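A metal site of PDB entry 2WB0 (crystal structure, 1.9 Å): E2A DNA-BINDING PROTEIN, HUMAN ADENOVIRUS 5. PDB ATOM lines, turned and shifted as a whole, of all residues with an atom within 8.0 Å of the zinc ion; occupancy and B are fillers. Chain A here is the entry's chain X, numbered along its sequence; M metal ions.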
ATOM      1  N   LYS A 110      -6.744  17.919 -16.462  1.00  0.00           N
ATOM      2  CA  LYS A 110      -5.975  19.100 -16.969  1.00  0.00           C
ATOM      3  C   LYS A 110      -5.185  19.693 -15.789  1.00  0.00           C
ATOM      4  O   LYS A 110      -5.675  19.719 -14.663  1.00  0.00           O
ATOM      5  CB  LYS A 110      -6.897  20.168 -17.604  1.00  0.00           C
ATOM      6  CG  LYS A 110      -7.551  19.590 -18.824  1.00  0.00           C
ATOM      7  CD  LYS A 110      -8.591  20.465 -19.419  1.00  0.00           C
ATOM      8  CE  LYS A 110      -9.550  19.603 -20.325  1.00  0.00           C
ATOM      9  NZ  LYS A 110     -10.760  18.637 -19.832  1.00  0.00           N
ATOM     10  N   CYS A 111      -3.945  20.120 -16.036  1.00  0.00           N
ATOM     11  CA  CYS A 111      -3.141  20.758 -15.008  1.00  0.00           C
ATOM     12  C   CYS A 111      -3.377  22.238 -14.936  1.00  0.00           C
ATOM     13  O   CYS A 111      -4.280  22.756 -15.578  1.00  0.00           O
ATOM     14  CB  CYS A 111      -1.647  20.448 -15.237  1.00  0.00           C
ATOM     15  SG  CYS A 111      -0.967  21.303 -16.653  1.00  0.00           S
ATOM     16  N   LEU A 112      -2.572  22.945 -14.131  1.00  0.00           N
ATOM     17  CA  LEU A 112      -2.729  24.395 -13.959  1.00  0.00           C
ATOM     18  C   LEU A 112      -2.480  25.199 -15.220  1.00  0.00           C
ATOM     19  O   LEU A 112      -3.035  26.277 -15.371  1.00  0.00           O
ATOM     20  CB  LEU A 112      -1.800  24.880 -12.852  1.00  0.00           C
ATOM     21  CG  LEU A 112      -2.240  24.928 -11.407  1.00  0.00           C
ATOM     22  CD1 LEU A 112      -3.724  24.580 -10.997  1.00  0.00           C
ATOM     23  CD2 LEU A 112      -1.149  24.544 -10.418  1.00  0.00           C
ATOM     24  N   HIS A 113      -1.741  24.634 -16.143  1.00  0.00           N
ATOM     25  CA  HIS A 113      -1.545  25.222 -17.440  1.00  0.00           C
ATOM     26  C   HIS A 113      -2.821  25.249 -18.247  1.00  0.00           C
ATOM     27  O   HIS A 113      -2.922  26.008 -19.224  1.00  0.00           O
ATOM     28  CB  HIS A 113      -0.558  24.425 -18.205  1.00  0.00           C
ATOM     29  CG  HIS A 113       0.845  24.657 -17.782  1.00  0.00           C
ATOM     30  ND1 HIS A 113       1.544  23.794 -16.957  1.00  0.00           N
ATOM     31  CD2 HIS A 113       1.694  25.668 -18.103  1.00  0.00           C
ATOM     32  CE1 HIS A 113       2.762  24.287 -16.763  1.00  0.00           C
ATOM     33  NE2 HIS A 113       2.862  25.423 -17.423  1.00  0.00           N
ATOM     34  N   GLY A 114      -3.774  24.393 -17.873  1.00  0.00           N
ATOM     35  CA  GLY A 114      -5.023  24.220 -18.595  1.00  0.00           C
ATOM     36  C   GLY A 114      -4.939  23.207 -19.736  1.00  0.00           C
ATOM     37  O   GLY A 114      -5.874  23.057 -20.533  1.00  0.00           O
ATOM     38  N   SER A 115      -3.811  22.518 -19.828  1.00  0.00           N
ATOM     39  CA  SER A 115      -3.612  21.477 -20.821  1.00  0.00           C
ATOM     40  C   SER A 115      -3.768  20.103 -20.221  1.00  0.00           C
ATOM     41  O   SER A 115      -3.581  19.872 -18.999  1.00  0.00           O
ATOM     42  CB  SER A 115      -2.226  21.587 -21.469  1.00  0.00           C
ATOM     43  OG  SER A 115      -1.202  21.780 -20.520  1.00  0.00           O
ATOM     44  N   ILE A 116      -4.192  19.198 -21.072  1.00  0.00           N
ATOM     45  CA  ILE A 116      -4.400  17.899 -20.615  1.00  0.00           C
ATOM     46  C   ILE A 116      -3.104  17.294 -20.062  1.00  0.00           C
ATOM     47  O   ILE A 116      -2.002  17.582 -20.586  1.00  0.00           O
ATOM     48  CB  ILE A 116      -5.106  16.972 -21.657  1.00  0.00           C
ATOM     49  CG1 ILE A 116      -4.219  16.019 -22.294  1.00  0.00           C
ATOM     50  CG2 ILE A 116      -6.260  17.484 -22.525  1.00  0.00           C
ATOM     51  CD1 ILE A 116      -4.553  14.905 -21.567  1.00  0.00           C
ATOM     52  N   MET A 117      -3.251  16.457 -19.016  1.00  0.00           N
ATOM     53  CA  MET A 117      -2.131  15.751 -18.396  1.00  0.00           C
ATOM     54  C   MET A 117      -1.843  14.404 -19.067  1.00  0.00           C
ATOM     55  O   MET A 117      -2.758  13.672 -19.379  1.00  0.00           O
ATOM     56  CB  MET A 117      -2.346  15.559 -16.860  1.00  0.00           C
ATOM     57  CG  MET A 117      -2.450  16.957 -16.129  1.00  0.00           C
ATOM     58  SD  MET A 117      -2.839  16.731 -14.329  1.00  0.00           S
ATOM     59  CE  MET A 117      -1.198  16.234 -13.719  1.00  0.00           C
ATOM     60  N   CYS A 165       0.995  13.423 -15.482  1.00  0.00           N
ATOM     61  CA  CYS A 165       1.932  14.535 -15.293  1.00  0.00           C
ATOM     62  C   CYS A 165       1.527  15.799 -16.116  1.00  0.00           C
ATOM     63  O   CYS A 165       0.765  15.726 -17.106  1.00  0.00           O
ATOM     64  CB  CYS A 165       3.354  14.064 -15.680  1.00  0.00           C
ATOM     65  SG  CYS A 165       3.610  13.815 -17.495  1.00  0.00           S
ATOM     66  N   CYS A 166       2.036  16.957 -15.704  1.00  0.00           N
ATOM     67  CA  CYS A 166       1.915  18.219 -16.469  1.00  0.00           C
ATOM     68  C   CYS A 166       2.550  17.934 -17.862  1.00  0.00           C
ATOM     69  O   CYS A 166       3.531  17.199 -17.909  1.00  0.00           O
ATOM     70  CB  CYS A 166       2.741  19.274 -15.759  1.00  0.00           C
ATOM     71  SG  CYS A 166       2.923  20.770 -16.734  1.00  0.00           S
ATOM     72  N   VAL A 167       2.024  18.452 -18.980  1.00  0.00           N
ATOM     73  CA  VAL A 167       2.648  18.054 -20.287  1.00  0.00           C
ATOM     74  C   VAL A 167       4.129  18.461 -20.383  1.00  0.00           C
ATOM     75  O   VAL A 167       4.946  17.781 -21.043  1.00  0.00           O
ATOM     76  CB  VAL A 167       1.829  18.570 -21.498  1.00  0.00           C
ATOM     77  CG1 VAL A 167       1.822  20.102 -21.537  1.00  0.00           C
ATOM     78  CG2 VAL A 167       2.375  17.948 -22.755  1.00  0.00           C
ATOM     79  N   HIS A 168       4.501  19.525 -19.655  1.00  0.00           N
ATOM     80  CA  HIS A 168       5.869  20.027 -19.701  1.00  0.00           C
ATOM     81  C   HIS A 168       6.823  19.110 -18.977  1.00  0.00           C
ATOM     82  O   HIS A 168       8.043  19.234 -19.152  1.00  0.00           O
ATOM     83  CB  HIS A 168       5.899  21.416 -19.093  1.00  0.00           C
ATOM     84  CG  HIS A 168       5.020  22.373 -19.832  1.00  0.00           C
ATOM     85  ND1 HIS A 168       5.463  23.104 -20.907  1.00  0.00           N
ATOM     86  CD2 HIS A 168       3.716  22.708 -19.660  1.00  0.00           C
ATOM     87  CE1 HIS A 168       4.472  23.861 -21.365  1.00  0.00           C
ATOM     88  NE2 HIS A 168       3.405  23.634 -20.618  1.00  0.00           N
ATOM     89  N   ASP A 169       6.283  18.143 -18.264  1.00  0.00           N
ATOM     90  CA  ASP A 169       7.061  17.078 -17.644  1.00  0.00           C
ATOM     91  C   ASP A 169       7.059  15.775 -18.389  1.00  0.00           C
ATOM     92  O   ASP A 169       7.533  14.782 -17.844  1.00  0.00           O
ATOM     93  CB  ASP A 169       6.575  16.879 -16.185  1.00  0.00           C
ATOM     94  CG  ASP A 169       6.741  18.170 -15.326  1.00  0.00           C
ATOM     95  OD1 ASP A 169       7.705  18.967 -15.616  1.00  0.00           O
ATOM     96  OD2 ASP A 169       5.926  18.399 -14.397  1.00  0.00           O
ATOM     97  N   LYS A 180       9.691  24.048 -16.377  1.00  0.00           N
ATOM     98  CA  LYS A 180       8.467  24.636 -16.956  1.00  0.00           C
ATOM     99  C   LYS A 180       7.208  24.017 -16.369  1.00  0.00           C
ATOM    100  O   LYS A 180       6.097  24.340 -16.827  1.00  0.00           O
ATOM    101  CB  LYS A 180       8.461  24.415 -18.463  1.00  0.00           C
ATOM    102  CG  LYS A 180       9.557  25.282 -19.194  1.00  0.00           C
ATOM    103  CD  LYS A 180       9.540  24.970 -20.677  1.00  0.00           C
ATOM    104  CE  LYS A 180      10.629  25.796 -21.444  1.00  0.00           C
ATOM    105  NZ  LYS A 180      10.530  27.231 -21.017  1.00  0.00           N
ATOM    106  N   SER A 181       7.370  23.140 -15.385  1.00  0.00           N
ATOM    107  CA  SER A 181       6.214  22.466 -14.770  1.00  0.00           C
ATOM    108  C   SER A 181       5.348  23.422 -13.987  1.00  0.00           C
ATOM    109  O   SER A 181       5.829  24.475 -13.557  1.00  0.00           O
ATOM    110  CB  SER A 181       6.703  21.433 -13.751  1.00  0.00           C
ATOM    111  OG  SER A 181       5.597  20.685 -13.261  1.00  0.00           O
ATOM    112  N   CYS A 182       4.055  23.076 -13.811  1.00  0.00           N
ATOM    113  CA  CYS A 182       3.176  23.739 -12.850  1.00  0.00           C
ATOM    114  C   CYS A 182       3.234  23.012 -11.493  1.00  0.00           C
ATOM    115  O   CYS A 182       2.677  23.525 -10.513  1.00  0.00           O
ATOM    116  CB  CYS A 182       1.695  23.797 -13.351  1.00  0.00           C
ATOM    117  SG  CYS A 182       1.031  22.153 -13.663  1.00  0.00           S
ATOM    118  N   GLY A 183       3.928  21.871 -11.439  1.00  0.00           N
ATOM    119  CA  GLY A 183       4.144  21.114 -10.205  1.00  0.00           C
ATOM    120  C   GLY A 183       3.021  20.116  -9.885  1.00  0.00           C
ATOM    121  O   GLY A 183       3.025  19.479  -8.849  1.00  0.00           O
ATOM    122  N   MET A 184       2.015  20.023 -10.751  1.00  0.00           N
ATOM    123  CA  MET A 184       0.918  19.092 -10.536  1.00  0.00           C
ATOM    124  C   MET A 184       1.306  17.712 -11.089  1.00  0.00           C
ATOM    125  O   MET A 184       1.869  17.588 -12.202  1.00  0.00           O
ATOM    126  CB  MET A 184      -0.313  19.620 -11.270  1.00  0.00           C
ATOM    127  CG  MET A 184      -1.593  18.987 -10.820  1.00  0.00           C
ATOM    128  SD  MET A 184      -3.048  20.007 -11.195  1.00  0.00           S
ATOM    129  CE  MET A 184      -2.631  21.544 -10.686  1.00  0.00           C
ATOM    130  N   PHE A 185       0.990  16.683 -10.327  1.00  0.00           N
ATOM    131  CA  PHE A 185       1.255  15.268 -10.668  1.00  0.00           C
ATOM    132  C   PHE A 185       0.295  14.411  -9.853  1.00  0.00           C
ATOM    133  O   PHE A 185       0.101  14.662  -8.625  1.00  0.00           O
ATOM    134  CB  PHE A 185       2.692  14.878 -10.324  1.00  0.00           C
ATOM    135  CG  PHE A 185       2.956  13.436 -10.522  1.00  0.00           C
ATOM    136  CD1 PHE A 185       3.182  12.948 -11.816  1.00  0.00           C
ATOM    137  CD2 PHE A 185       2.848  12.537  -9.438  1.00  0.00           C
ATOM    138  CE1 PHE A 185       3.412  11.575 -12.046  1.00  0.00           C
ATOM    139  CE2 PHE A 185       3.109  11.146  -9.677  1.00  0.00           C
ATOM    140  CZ  PHE A 185       3.367  10.699 -10.953  1.00  0.00           C
ATOM    141  N   TRP A 331      -2.762  31.015 -15.630  1.00  0.00           N
ATOM    142  CA  TRP A 331      -1.406  30.480 -15.555  1.00  0.00           C
ATOM    143  C   TRP A 331      -0.438  31.631 -15.826  1.00  0.00           C
ATOM    144  O   TRP A 331      -0.693  32.436 -16.726  1.00  0.00           O
ATOM    145  CB  TRP A 331      -1.152  29.349 -16.605  1.00  0.00           C
ATOM    146  CG  TRP A 331       0.297  28.975 -16.522  1.00  0.00           C
ATOM    147  CD1 TRP A 331       1.318  29.255 -17.415  1.00  0.00           C
ATOM    148  CD2 TRP A 331       0.900  28.294 -15.416  1.00  0.00           C
ATOM    149  NE1 TRP A 331       2.520  28.813 -16.896  1.00  0.00           N
ATOM    150  CE2 TRP A 331       2.284  28.215 -15.666  1.00  0.00           C
ATOM    151  CE3 TRP A 331       0.400  27.791 -14.189  1.00  0.00           C
ATOM    152  CZ2 TRP A 331       3.164  27.623 -14.767  1.00  0.00           C
ATOM    153  CZ3 TRP A 331       1.315  27.176 -13.281  1.00  0.00           C
ATOM    154  CH2 TRP A 331       2.663  27.130 -13.592  1.00  0.00           C
HETATM  155 ZN    ZN M   1       1.082  22.032 -16.001  1.00  0.00          ZN
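Of the 20 residues printed, 4 come within 4 Å of the zinc ion.
The zinc ion is bound by a ring nitrogen (ND1) of His 113 (2.1 Å), the side-chain sulfur of Cys 111 (2.3 Å), the side-chain sulfur of Cys 182 (2.3 Å) and the side-chain sulfur of Cys 166 (2.3 Å).
NE2 of His 113 lies close to O of Lys 180 (3.5 Å).
The indole nitrogen of Trp 331 sits close to a ring nitrogen (NE2) of His 113.
The side-chain sulfur (SG) of Cys 111 sits close to the backbone carbonyl oxygen (O) of Ser 115 (3.8 Å).
The side-chain sulfur (SG) of Cys 182 lies close to the backbone NH (N) of Leu 112, at 3.7 Å.
The backbone NH of Met 184 sits close to the side-chain sulfur of Cys 182.
SG of Cys 166 sits close to N of His 168 (3.5 Å).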
